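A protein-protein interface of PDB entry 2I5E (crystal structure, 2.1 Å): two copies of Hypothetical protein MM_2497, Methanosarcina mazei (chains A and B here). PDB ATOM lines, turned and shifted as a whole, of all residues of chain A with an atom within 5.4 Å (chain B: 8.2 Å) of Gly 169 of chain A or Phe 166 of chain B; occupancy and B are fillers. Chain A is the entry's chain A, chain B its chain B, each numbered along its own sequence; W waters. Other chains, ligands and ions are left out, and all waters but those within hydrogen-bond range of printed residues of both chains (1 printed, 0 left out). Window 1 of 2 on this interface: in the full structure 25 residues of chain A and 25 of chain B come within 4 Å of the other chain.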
ATOM      1  N   VAL A 119     -21.283  18.534 -27.398  1.00  0.00           N
ATOM      2  CA  VAL A 119     -21.806  19.504 -26.445  1.00  0.00           C
ATOM      3  C   VAL A 119     -22.738  20.576 -27.075  1.00  0.00           C
ATOM      4  O   VAL A 119     -22.281  21.412 -27.905  1.00  0.00           O
ATOM      5  CB  VAL A 119     -20.618  20.265 -25.783  1.00  0.00           C
ATOM      6  CG1 VAL A 119     -21.068  21.020 -24.530  1.00  0.00           C
ATOM      7  CG2 VAL A 119     -19.533  19.233 -25.462  1.00  0.00           C
ATOM      8  N   PRO A 120     -24.040  20.550 -26.691  1.00  0.00           N
ATOM      9  CA  PRO A 120     -25.011  21.492 -27.234  1.00  0.00           C
ATOM     10  C   PRO A 120     -24.720  22.843 -26.674  1.00  0.00           C
ATOM     11  O   PRO A 120     -24.197  22.939 -25.540  1.00  0.00           O
ATOM     12  CB  PRO A 120     -26.355  21.006 -26.721  1.00  0.00           C
ATOM     13  CG  PRO A 120     -26.053  20.074 -25.520  1.00  0.00           C
ATOM     14  CD  PRO A 120     -24.621  19.624 -25.677  1.00  0.00           C
ATOM     15  N   GLY A 121     -25.013  23.893 -27.448  1.00  0.00           N
ATOM     16  CA  GLY A 121     -25.119  25.173 -26.841  1.00  0.00           C
ATOM     17  C   GLY A 121     -26.573  25.594 -26.905  1.00  0.00           C
ATOM     18  O   GLY A 121     -27.463  24.789 -27.268  1.00  0.00           O
ATOM     19  N   LYS A 122     -26.882  26.826 -26.487  1.00  0.00           N
ATOM     20  CA  LYS A 122     -28.351  27.154 -26.651  1.00  0.00           C
ATOM     21  C   LYS A 122     -28.832  27.359 -28.120  1.00  0.00           C
ATOM     22  O   LYS A 122     -28.018  27.555 -29.033  1.00  0.00           O
ATOM     23  CB  LYS A 122     -28.868  28.243 -25.745  1.00  0.00           C
ATOM     24  CG  LYS A 122     -28.196  29.523 -25.974  1.00  0.00           C
ATOM     25  CD  LYS A 122     -28.966  30.686 -25.237  1.00  0.00           C
ATOM     26  CE  LYS A 122     -27.928  31.819 -24.896  1.00  0.00           C
ATOM     27  NZ  LYS A 122     -26.610  31.741 -25.806  1.00  0.00           N
ATOM     28  N   ASN A 127     -21.286  23.608 -29.136  1.00  0.00           N
ATOM     29  CA  ASN A 127     -20.276  24.367 -28.392  1.00  0.00           C
ATOM     30  C   ASN A 127     -18.904  23.683 -28.403  1.00  0.00           C
ATOM     31  O   ASN A 127     -17.889  24.356 -28.318  1.00  0.00           O
ATOM     32  CB  ASN A 127     -20.748  24.613 -26.922  1.00  0.00           C
ATOM     33  CG  ASN A 127     -21.677  25.851 -26.819  1.00  0.00           C
ATOM     34  OD1 ASN A 127     -21.835  26.608 -27.783  1.00  0.00           O
ATOM     35  ND2 ASN A 127     -22.260  26.050 -25.675  1.00  0.00           N
ATOM     36  N   ASP A 164     -23.761  16.213 -21.452  1.00  0.00           N
ATOM     37  CA  ASP A 164     -24.845  16.962 -20.841  1.00  0.00           C
ATOM     38  C   ASP A 164     -24.316  17.797 -19.697  1.00  0.00           C
ATOM     39  O   ASP A 164     -24.314  17.367 -18.572  1.00  0.00           O
ATOM     40  CB  ASP A 164     -25.918  15.981 -20.321  1.00  0.00           C
ATOM     41  CG  ASP A 164     -26.988  16.681 -19.509  1.00  0.00           C
ATOM     42  OD1 ASP A 164     -27.334  17.853 -19.824  1.00  0.00           O
ATOM     43  OD2 ASP A 164     -27.464  16.106 -18.517  1.00  0.00           O
ATOM     44  N   SER A 165     -23.907  19.024 -19.967  1.00  0.00           N
ATOM     45  CA  SER A 165     -23.285  19.871 -19.003  1.00  0.00           C
ATOM     46  C   SER A 165     -23.915  21.261 -19.183  1.00  0.00           C
ATOM     47  O   SER A 165     -23.798  21.829 -20.247  1.00  0.00           O
ATOM     48  CB  SER A 165     -21.801  20.044 -19.404  1.00  0.00           C
ATOM     49  OG  SER A 165     -21.217  20.996 -18.555  1.00  0.00           O
ATOM     50  N   PHE A 166     -24.407  21.848 -18.102  1.00  0.00           N
ATOM     51  CA  PHE A 166     -24.884  23.210 -18.028  1.00  0.00           C
ATOM     52  C   PHE A 166     -23.694  24.176 -18.305  1.00  0.00           C
ATOM     53  O   PHE A 166     -23.867  25.195 -18.978  1.00  0.00           O
ATOM     54  CB  PHE A 166     -25.489  23.450 -16.604  1.00  0.00           C
ATOM     55  CG  PHE A 166     -26.271  24.765 -16.426  1.00  0.00           C
ATOM     56  CD1 PHE A 166     -27.635  24.768 -16.333  1.00  0.00           C
ATOM     57  CD2 PHE A 166     -25.618  25.986 -16.324  1.00  0.00           C
ATOM     58  CE1 PHE A 166     -28.343  25.976 -16.101  1.00  0.00           C
ATOM     59  CE2 PHE A 166     -26.297  27.191 -16.165  1.00  0.00           C
ATOM     60  CZ  PHE A 166     -27.639  27.192 -16.037  1.00  0.00           C
ATOM     61  N   MET A 167     -22.528  23.916 -17.717  1.00  0.00           N
ATOM     62  CA  MET A 167     -21.443  24.894 -17.767  1.00  0.00           C
ATOM     63  C   MET A 167     -20.834  24.900 -19.181  1.00  0.00           C
ATOM     64  O   MET A 167     -20.594  25.964 -19.723  1.00  0.00           O
ATOM     65  CB  MET A 167     -20.361  24.569 -16.768  1.00  0.00           C
ATOM     66  CG  MET A 167     -20.804  24.591 -15.283  1.00  0.00           C
ATOM     67  SD  MET A 167     -21.584  26.236 -14.661  1.00  0.00           S
ATOM     68  CE  MET A 167     -23.239  25.469 -13.772  1.00  0.00           C
ATOM     69  N   ALA A 168     -20.612  23.723 -19.787  1.00  0.00           N
ATOM     70  CA  ALA A 168     -19.997  23.682 -21.110  1.00  0.00           C
ATOM     71  C   ALA A 168     -21.069  24.074 -22.177  1.00  0.00           C
ATOM     72  O   ALA A 168     -20.765  24.414 -23.321  1.00  0.00           O
ATOM     73  CB  ALA A 168     -19.427  22.217 -21.416  1.00  0.00           C
ATOM     74  N   GLY A 169     -22.324  24.018 -21.798  1.00  0.00           N
ATOM     75  CA  GLY A 169     -23.361  24.466 -22.690  1.00  0.00           C
ATOM     76  C   GLY A 169     -23.798  25.913 -22.644  1.00  0.00           C
ATOM     77  O   GLY A 169     -24.630  26.319 -23.454  1.00  0.00           O
ATOM     78  N   THR A 170     -23.221  26.702 -21.729  1.00  0.00           N
ATOM     79  CA  THR A 170     -23.432  28.176 -21.645  1.00  0.00           C
ATOM     80  C   THR A 170     -22.401  28.887 -22.487  1.00  0.00           C
ATOM     81  O   THR A 170     -21.255  29.164 -22.059  1.00  0.00           O
ATOM     82  CB  THR A 170     -23.349  28.579 -20.184  1.00  0.00           C
ATOM     83  OG1 THR A 170     -24.287  27.762 -19.483  1.00  0.00           O
ATOM     84  CG2 THR A 170     -23.722  30.037 -19.911  1.00  0.00           C
ATOM     85  N   ASP A 171     -22.790  29.157 -23.735  1.00  0.00           N
ATOM     86  CA  ASP A 171     -22.019  30.021 -24.597  1.00  0.00           C
ATOM     87  C   ASP A 171     -22.560  31.427 -24.345  1.00  0.00           C
ATOM     88  O   ASP A 171     -23.734  31.626 -24.002  1.00  0.00           O
ATOM     89  CB  ASP A 171     -22.161  29.635 -26.058  1.00  0.00           C
ATOM     90  CG  ASP A 171     -23.624  29.442 -26.492  1.00  0.00           C
ATOM     91  OD1 ASP A 171     -24.270  28.472 -26.086  1.00  0.00           O
ATOM     92  OD2 ASP A 171     -24.127  30.303 -27.199  1.00  0.00           O
ATOM     93  N   LEU B 100     -37.006  17.930 -19.950  1.00  0.00           N
ATOM     94  CA  LEU B 100     -35.777  17.254 -20.362  1.00  0.00           C
ATOM     95  C   LEU B 100     -35.087  16.452 -19.251  1.00  0.00           C
ATOM     96  O   LEU B 100     -34.126  15.732 -19.449  1.00  0.00           O
ATOM     97  CB  LEU B 100     -34.843  18.303 -20.972  1.00  0.00           C
ATOM     98  CG  LEU B 100     -35.330  19.177 -22.174  1.00  0.00           C
ATOM     99  CD1 LEU B 100     -34.083  19.962 -22.754  1.00  0.00           C
ATOM    100  CD2 LEU B 100     -35.868  18.417 -23.276  1.00  0.00           C
ATOM    101  N   LEU B 101     -35.625  16.557 -18.047  1.00  0.00           N
ATOM    102  CA  LEU B 101     -35.175  15.823 -16.882  1.00  0.00           C
ATOM    103  C   LEU B 101     -35.462  14.313 -17.066  1.00  0.00           C
ATOM    104  O   LEU B 101     -36.606  13.984 -17.350  1.00  0.00           O
ATOM    105  CB  LEU B 101     -35.967  16.329 -15.679  1.00  0.00           C
ATOM    106  CG  LEU B 101     -35.442  15.747 -14.350  1.00  0.00           C
ATOM    107  CD1 LEU B 101     -34.152  16.372 -14.033  1.00  0.00           C
ATOM    108  CD2 LEU B 101     -36.474  16.040 -13.229  1.00  0.00           C
ATOM    109  N   HIS B 105     -31.096  11.407 -14.510  1.00  0.00           N
ATOM    110  CA  HIS B 105     -30.754  12.648 -13.782  1.00  0.00           C
ATOM    111  C   HIS B 105     -31.251  12.499 -12.365  1.00  0.00           C
ATOM    112  O   HIS B 105     -30.594  12.936 -11.451  1.00  0.00           O
ATOM    113  CB  HIS B 105     -31.457  13.944 -14.339  1.00  0.00           C
ATOM    114  CG  HIS B 105     -31.112  14.267 -15.745  1.00  0.00           C
ATOM    115  ND1 HIS B 105     -29.815  14.327 -16.216  1.00  0.00           N
ATOM    116  CD2 HIS B 105     -31.895  14.545 -16.796  1.00  0.00           C
ATOM    117  CE1 HIS B 105     -29.825  14.583 -17.506  1.00  0.00           C
ATOM    118  NE2 HIS B 105     -31.076  14.701 -17.882  1.00  0.00           N
ATOM    119  N   VAL B 119     -29.514  21.729  -8.462  1.00  0.00           N
ATOM    120  CA  VAL B 119     -29.525  21.870  -9.939  1.00  0.00           C
ATOM    121  C   VAL B 119     -29.945  23.314 -10.259  1.00  0.00           C
ATOM    122  O   VAL B 119     -31.067  23.711  -9.952  1.00  0.00           O
ATOM    123  CB  VAL B 119     -30.549  20.873 -10.606  1.00  0.00           C
ATOM    124  CG1 VAL B 119     -30.545  20.967 -12.091  1.00  0.00           C
ATOM    125  CG2 VAL B 119     -30.232  19.488 -10.227  1.00  0.00           C
ATOM    126  N   PRO B 120     -29.065  24.100 -10.924  1.00  0.00           N
ATOM    127  CA  PRO B 120     -29.505  25.408 -11.323  1.00  0.00           C
ATOM    128  C   PRO B 120     -30.467  25.462 -12.535  1.00  0.00           C
ATOM    129  O   PRO B 120     -30.491  24.604 -13.344  1.00  0.00           O
ATOM    130  CB  PRO B 120     -28.215  26.132 -11.665  1.00  0.00           C
ATOM    131  CG  PRO B 120     -27.271  24.929 -12.307  1.00  0.00           C
ATOM    132  CD  PRO B 120     -27.694  23.755 -11.378  1.00  0.00           C
ATOM    133  N   GLY B 121     -31.303  26.488 -12.583  1.00  0.00           N
ATOM    134  CA  GLY B 121     -32.023  26.801 -13.762  1.00  0.00           C
ATOM    135  C   GLY B 121     -31.484  28.021 -14.463  1.00  0.00           C
ATOM    136  O   GLY B 121     -30.452  28.655 -14.063  1.00  0.00           O
ATOM    137  N   LYS B 122     -32.182  28.367 -15.557  1.00  0.00           N
ATOM    138  CA  LYS B 122     -31.862  29.582 -16.289  1.00  0.00           C
ATOM    139  C   LYS B 122     -31.980  30.807 -15.381  1.00  0.00           C
ATOM    140  O   LYS B 122     -32.843  30.859 -14.538  1.00  0.00           O
ATOM    141  CB  LYS B 122     -32.796  29.749 -17.492  1.00  0.00           C
ATOM    142  CG  LYS B 122     -32.400  30.866 -18.434  1.00  0.00           C
ATOM    143  CD  LYS B 122     -33.515  31.117 -19.591  1.00  0.00           C
ATOM    144  CE  LYS B 122     -35.018  31.226 -19.041  1.00  0.00           C
ATOM    145  NZ  LYS B 122     -35.909  29.929 -18.572  1.00  0.00           N
ATOM    146  N   ASN B 127     -33.856  24.514 -10.163  1.00  0.00           N
ATOM    147  CA  ASN B 127     -34.783  23.604 -10.816  1.00  0.00           C
ATOM    148  C   ASN B 127     -35.104  22.382  -9.981  1.00  0.00           C
ATOM    149  O   ASN B 127     -36.225  21.818 -10.023  1.00  0.00           O
ATOM    150  CB  ASN B 127     -34.208  23.221 -12.211  1.00  0.00           C
ATOM    151  CG  ASN B 127     -34.519  24.277 -13.245  1.00  0.00           C
ATOM    152  OD1 ASN B 127     -35.193  25.352 -12.954  1.00  0.00           O
ATOM    153  ND2 ASN B 127     -34.005  24.058 -14.426  1.00  0.00           N
ATOM    154  N   TYR B 163     -25.192  19.973  -9.337  1.00  0.00           N
ATOM    155  CA  TYR B 163     -25.341  18.994 -10.393  1.00  0.00           C
ATOM    156  C   TYR B 163     -25.282  19.708 -11.763  1.00  0.00           C
ATOM    157  O   TYR B 163     -26.057  20.600 -12.030  1.00  0.00           O
ATOM    158  CB  TYR B 163     -26.657  18.324 -10.244  1.00  0.00           C
ATOM    159  CG  TYR B 163     -26.796  17.155 -11.127  1.00  0.00           C
ATOM    160  CD1 TYR B 163     -26.043  15.988 -10.925  1.00  0.00           C
ATOM    161  CD2 TYR B 163     -27.755  17.170 -12.135  1.00  0.00           C
ATOM    162  CE1 TYR B 163     -26.217  14.877 -11.773  1.00  0.00           C
ATOM    163  CE2 TYR B 163     -27.949  16.082 -12.972  1.00  0.00           C
ATOM    164  CZ  TYR B 163     -27.183  14.963 -12.824  1.00  0.00           C
ATOM    165  OH  TYR B 163     -27.466  13.922 -13.685  1.00  0.00           O
ATOM    166  N   ASP B 164     -24.349  19.337 -12.615  1.00  0.00           N
ATOM    167  CA  ASP B 164     -24.047  20.163 -13.783  1.00  0.00           C
ATOM    168  C   ASP B 164     -24.768  19.506 -14.946  1.00  0.00           C
ATOM    169  O   ASP B 164     -24.280  18.602 -15.526  1.00  0.00           O
ATOM    170  CB  ASP B 164     -22.515  20.243 -14.007  1.00  0.00           C
ATOM    171  CG  ASP B 164     -22.129  20.889 -15.346  1.00  0.00           C
ATOM    172  OD1 ASP B 164     -22.892  21.801 -15.801  1.00  0.00           O
ATOM    173  OD2 ASP B 164     -21.078  20.488 -15.922  1.00  0.00           O
ATOM    174  N   SER B 165     -25.995  19.920 -15.228  1.00  0.00           N
ATOM    175  CA  SER B 165     -26.757  19.280 -16.281  1.00  0.00           C
ATOM    176  C   SER B 165     -27.504  20.312 -17.197  1.00  0.00           C
ATOM    177  O   SER B 165     -28.235  21.169 -16.742  1.00  0.00           O
ATOM    178  CB  SER B 165     -27.755  18.307 -15.639  1.00  0.00           C
ATOM    179  OG  SER B 165     -28.652  17.844 -16.592  1.00  0.00           O
ATOM    180  N   PHE B 166     -27.318  20.179 -18.500  1.00  0.00           N
ATOM    181  CA  PHE B 166     -27.929  21.078 -19.471  1.00  0.00           C
ATOM    182  C   PHE B 166     -29.400  20.793 -19.506  1.00  0.00           C
ATOM    183  O   PHE B 166     -30.235  21.718 -19.525  1.00  0.00           O
ATOM    184  CB  PHE B 166     -27.275  20.773 -20.798  1.00  0.00           C
ATOM    185  CG  PHE B 166     -27.742  21.630 -21.927  1.00  0.00           C
ATOM    186  CD1 PHE B 166     -27.085  22.807 -22.246  1.00  0.00           C
ATOM    187  CD2 PHE B 166     -28.908  21.281 -22.690  1.00  0.00           C
ATOM    188  CE1 PHE B 166     -27.522  23.580 -23.346  1.00  0.00           C
ATOM    189  CE2 PHE B 166     -29.341  22.081 -23.751  1.00  0.00           C
ATOM    190  CZ  PHE B 166     -28.637  23.248 -24.052  1.00  0.00           C
ATOM    191  N   MET B 167     -29.738  19.508 -19.578  1.00  0.00           N
ATOM    192  CA  MET B 167     -31.118  19.023 -19.738  1.00  0.00           C
ATOM    193  C   MET B 167     -31.980  19.311 -18.506  1.00  0.00           C
ATOM    194  O   MET B 167     -33.079  19.827 -18.636  1.00  0.00           O
ATOM    195  CB  MET B 167     -31.073  17.540 -19.954  1.00  0.00           C
ATOM    196  CG  MET B 167     -30.393  17.162 -21.184  1.00  0.00           C
ATOM    197  SD  MET B 167     -30.916  17.941 -22.877  1.00  0.00           S
ATOM    198  CE  MET B 167     -29.065  18.036 -23.680  1.00  0.00           C
ATOM    199  N   ALA B 168     -31.419  19.061 -17.330  1.00  0.00           N
ATOM    200  CA  ALA B 168     -32.003  19.362 -16.022  1.00  0.00           C
ATOM    201  C   ALA B 168     -32.093  20.852 -15.749  1.00  0.00           C
ATOM    202  O   ALA B 168     -33.014  21.340 -14.974  1.00  0.00           O
ATOM    203  CB  ALA B 168     -31.156  18.648 -14.871  1.00  0.00           C
ATOM    204  N   GLY B 169     -31.165  21.568 -16.393  1.00  0.00           N
ATOM    205  CA  GLY B 169     -31.092  22.952 -16.283  1.00  0.00           C
ATOM    206  C   GLY B 169     -32.073  23.699 -17.185  1.00  0.00           C
ATOM    207  O   GLY B 169     -32.177  24.947 -17.035  1.00  0.00           O
ATOM    208  N   THR B 170     -32.854  22.951 -17.998  1.00  0.00           N
ATOM    209  CA  THR B 170     -33.700  23.565 -19.022  1.00  0.00           C
ATOM    210  C   THR B 170     -35.125  23.616 -18.486  1.00  0.00           C
ATOM    211  O   THR B 170     -35.940  22.695 -18.660  1.00  0.00           O
ATOM    212  CB  THR B 170     -33.636  22.805 -20.406  1.00  0.00           C
ATOM    213  OG1 THR B 170     -32.294  22.811 -20.920  1.00  0.00           O
ATOM    214  CG2 THR B 170     -34.544  23.442 -21.468  1.00  0.00           C
ATOM    215  N   ASP B 171     -35.433  24.700 -17.779  1.00  0.00           N
ATOM    216  CA  ASP B 171     -36.781  24.913 -17.322  1.00  0.00           C
ATOM    217  C   ASP B 171     -37.509  25.627 -18.452  1.00  0.00           C
ATOM    218  O   ASP B 171     -36.914  26.400 -19.195  1.00  0.00           O
ATOM    219  CB  ASP B 171     -36.804  25.721 -16.016  1.00  0.00           C
ATOM    220  CG  ASP B 171     -36.000  27.051 -16.050  1.00  0.00           C
ATOM    221  OD1 ASP B 171     -34.736  27.048 -16.008  1.00  0.00           O
ATOM    222  OD2 ASP B 171     -36.646  28.121 -15.905  1.00  0.00           O
ATOM    223  N   GLU B 180     -35.708  24.806 -27.146  1.00  0.00           N
ATOM    224  CA  GLU B 180     -34.826  23.814 -26.551  1.00  0.00           C
ATOM    225  C   GLU B 180     -35.592  22.528 -26.494  1.00  0.00           C
ATOM    226  O   GLU B 180     -35.071  21.372 -26.600  1.00  0.00           O
ATOM    227  CB  GLU B 180     -34.422  24.223 -25.089  1.00  0.00           C
ATOM    228  CG  GLU B 180     -33.679  25.568 -24.970  1.00  0.00           C
ATOM    229  CD  GLU B 180     -32.287  25.526 -25.679  1.00  0.00           C
ATOM    230  OE1 GLU B 180     -31.747  24.462 -25.979  1.00  0.00           O
ATOM    231  OE2 GLU B 180     -31.810  26.559 -26.045  1.00  0.00           O
ATOM    232  N   LEU B 181     -36.884  22.683 -26.219  1.00  0.00           N
ATOM    233  CA  LEU B 181     -37.690  21.480 -25.945  1.00  0.00           C
ATOM    234  C   LEU B 181     -37.776  20.719 -27.264  1.00  0.00           C
ATOM    235  O   LEU B 181     -37.751  19.445 -27.308  1.00  0.00           O
ATOM    236  CB  LEU B 181     -39.094  21.925 -25.361  1.00  0.00           C
ATOM    237  CG  LEU B 181     -40.208  20.857 -25.290  1.00  0.00           C
ATOM    238  CD1 LEU B 181     -39.679  19.687 -24.576  1.00  0.00           C
ATOM    239  CD2 LEU B 181     -41.396  21.341 -24.472  1.00  0.00           C
ATOM    240  N   ILE B 183     -35.802  20.816 -29.888  1.00  0.00           N
ATOM    241  CA  ILE B 183     -34.509  20.211 -30.268  1.00  0.00           C
ATOM    242  C   ILE B 183     -34.207  18.959 -29.471  1.00  0.00           C
ATOM    243  O   ILE B 183     -33.780  17.956 -30.023  1.00  0.00           O
ATOM    244  CB  ILE B 183     -33.343  21.217 -30.018  1.00  0.00           C
ATOM    245  CG1 ILE B 183     -33.492  22.539 -30.813  1.00  0.00           C
ATOM    246  CG2 ILE B 183     -31.959  20.589 -30.226  1.00  0.00           C
ATOM    247  CD1 ILE B 183     -33.199  22.380 -32.300  1.00  0.00           C
ATOM    248  N   HIS B 184     -34.404  19.013 -28.151  1.00  0.00           N
ATOM    249  CA  HIS B 184     -33.878  17.985 -27.240  1.00  0.00           C
ATOM    250  C   HIS B 184     -34.916  17.037 -26.619  1.00  0.00           C
ATOM    251  O   HIS B 184     -34.501  16.095 -26.005  1.00  0.00           O
ATOM    252  CB  HIS B 184     -33.128  18.714 -26.039  1.00  0.00           C
ATOM    253  CG  HIS B 184     -31.934  19.493 -26.467  1.00  0.00           C
ATOM    254  ND1 HIS B 184     -30.802  18.903 -27.001  1.00  0.00           N
ATOM    255  CD2 HIS B 184     -31.716  20.817 -26.508  1.00  0.00           C
ATOM    256  CE1 HIS B 184     -29.907  19.835 -27.263  1.00  0.00           C
ATOM    257  NE2 HIS B 184     -30.440  21.005 -26.992  1.00  0.00           N
HETATM  258  O   HOH W   1     -29.862  23.795 -27.652  1.00  0.00           O
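Of the 13 printed residues of chain A, 8 touch a printed residue of chain B. Hydrophobic or aromatic side chains of chain A within 4 Å of the printed part of chain B: Pro 120, Phe 166 and Met 167. Among the printed residues, 18 pairs touch across the chains. Among the printed residues, no Asp or Glu carboxylate lies within 4 Å of a Lys or Arg side-chain nitrogen of the other chain.
OD2 of Asp 171 of chain A lies within salt-bridge range of NZ of Lys 122 of chain A, 3.2 Å away. ND2 of Asn 127 of chain A lies within hydrogen-bond range of O of Gly 169 of chain A (3.3 Å). N of Met 167 of chain A lies within hydrogen-bond range of OG of Ser 165 of chain A, 3.3 Å away. A ring nitrogen (ND1) of His 105 of chain B is in hydrogen-bond range of the side-chain hydroxyl (OH) of Tyr 163 of chain B (3.5 Å). The side-chain hydroxyl (OG) of Ser 165 of chain B is in hydrogen-bond range of the backbone NH (N) of Ala 168 of chain B (3.1 Å). OG1 of Thr 170 of chain B lies within hydrogen-bond range of O of Phe 166 of chain B (2.7 Å).
Water W1 lies within hydrogen-bond range of the side-chain carboxylate (OE1) of Glu 180 of chain B (2.6 Å), the backbone carbonyl oxygen (O) of Gly 121 of chain A (2.6 Å) and a ring nitrogen (NE2) of His 184 of chain B (2.9 Å).
The side-chain hydroxyl (OG) of Ser 165 of chain B is in hydrogen-bond range of the side-chain carboxylate (OD2) of Asp 164 of chain A (2.9 Å). OD1 of Asp 164 of chain A is in hydrogen-bond range of N of Phe 166 of chain B, 2.7 Å away. The backbone NH (N) of Met 167 of chain B is in hydrogen-bond range of the side-chain carboxylate (OD1) of Asp 164 of chain A (2.9 Å). OD2 of Asp 164 of chain B lies within hydrogen-bond range of OG of Ser 165 of chain A. N of Phe 166 of chain A sits at hydrogen-bond distance from OD1 of Asp 164 of chain B (2.8 Å). The backbone NH (N) of Met 167 of chain A is in hydrogen-bond range of the side-chain carboxylate (OD1) of Asp 164 of chain B (2.9 Å). O of Asp 164 of chain B sits close to O of Asp 164 of chain A (3.3 Å). N of Phe 166 of chain A lies close to N of Phe 166 of chain B (3.4 Å).
CB of Pro 120 of chain A touches CE1 of His 184 of chain B (3.8 Å). Gly 121 of chain A touches Phe 166 of chain B (O to CZ, 3.8 Å). Glu 180 of chain B touches Lys 122 of chain A (OE2 to CB, 3.4 Å). OD2 of Asp 164 of chain A touches CE1 of His 105 of chain B, 3.0 Å away. Phe 166 of chain B touches Ser 165 of chain A (N to C, 3.6 Å). O of Pro 120 of chain B touches CE1 of Phe 166 of chain A, 3.8 Å away. O of Gly 121 of chain B touches CZ of Phe 166 of chain A, 3.7 Å away. Phe 166 of chain A touches Ser 165 of chain B. Gly 169 of chain B touches Phe 166 of chain A (CA to CD1, 3.9 Å). Phe 166 of chain B touches Gly 169 of chain A (CE1 to O, 3.98 Å).
Of the printed residues of chain B, Gly 169 of chain A touches Phe 166. Of the printed residues of chain A, Phe 166 of chain B touches Gly 121 (3.8 Å), Asp 164 (2.7 Å), Ser 165 (3.6 Å), Phe 166 (3.4 Å) and Gly 169 (3.98 Å). No residue of chain B comes within 4 Å of Ala 168 of chain A. Of the printed residues of chain A, Asp 164 of chain B touches Asp 164, Ser 165, Phe 166 and Met 167. Printed residues of chain B within 4 Å of Asp 164 of chain A: His 105, Asp 164, Ser 165, Phe 166 and Met 167. Leu 181 of chain B touches none of the printed residues of chain A. Asp 171 of chain B touches none of the printed residues of chain A. The nearest printed residue of chain A that does not touch Phe 166 of chain B is Pro 120 of chain A (4.03 Å). The nearest printed residue of chain A that does not touch Ser 165 of chain B is Ser 165 of chain A (4.2 Å).
Asp 164 of chain A touches Phe 166 of chain B, and with the chains exchanged Phe 166 of chain A touches Asp 164 of chain B. Asp 164 of chain A touches Met 167 of chain B, and with the chains exchanged Met 167 of chain A touches Asp 164 of chain B. Ser 165 of chain A touches Phe 166 of chain B, and with the chains exchanged Phe 166 of chain A touches Ser 165 of chain B. Phe 166 of chain A touches Pro 120 of chain B, but with the chains exchanged Pro 120 of chain A does not touch Phe 166 of chain B (4.03 Å). Positions printed for both chains: 119, 120, 121, 122, 127, 164, 165, 166, 167, 168, 169, 170 and 171.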
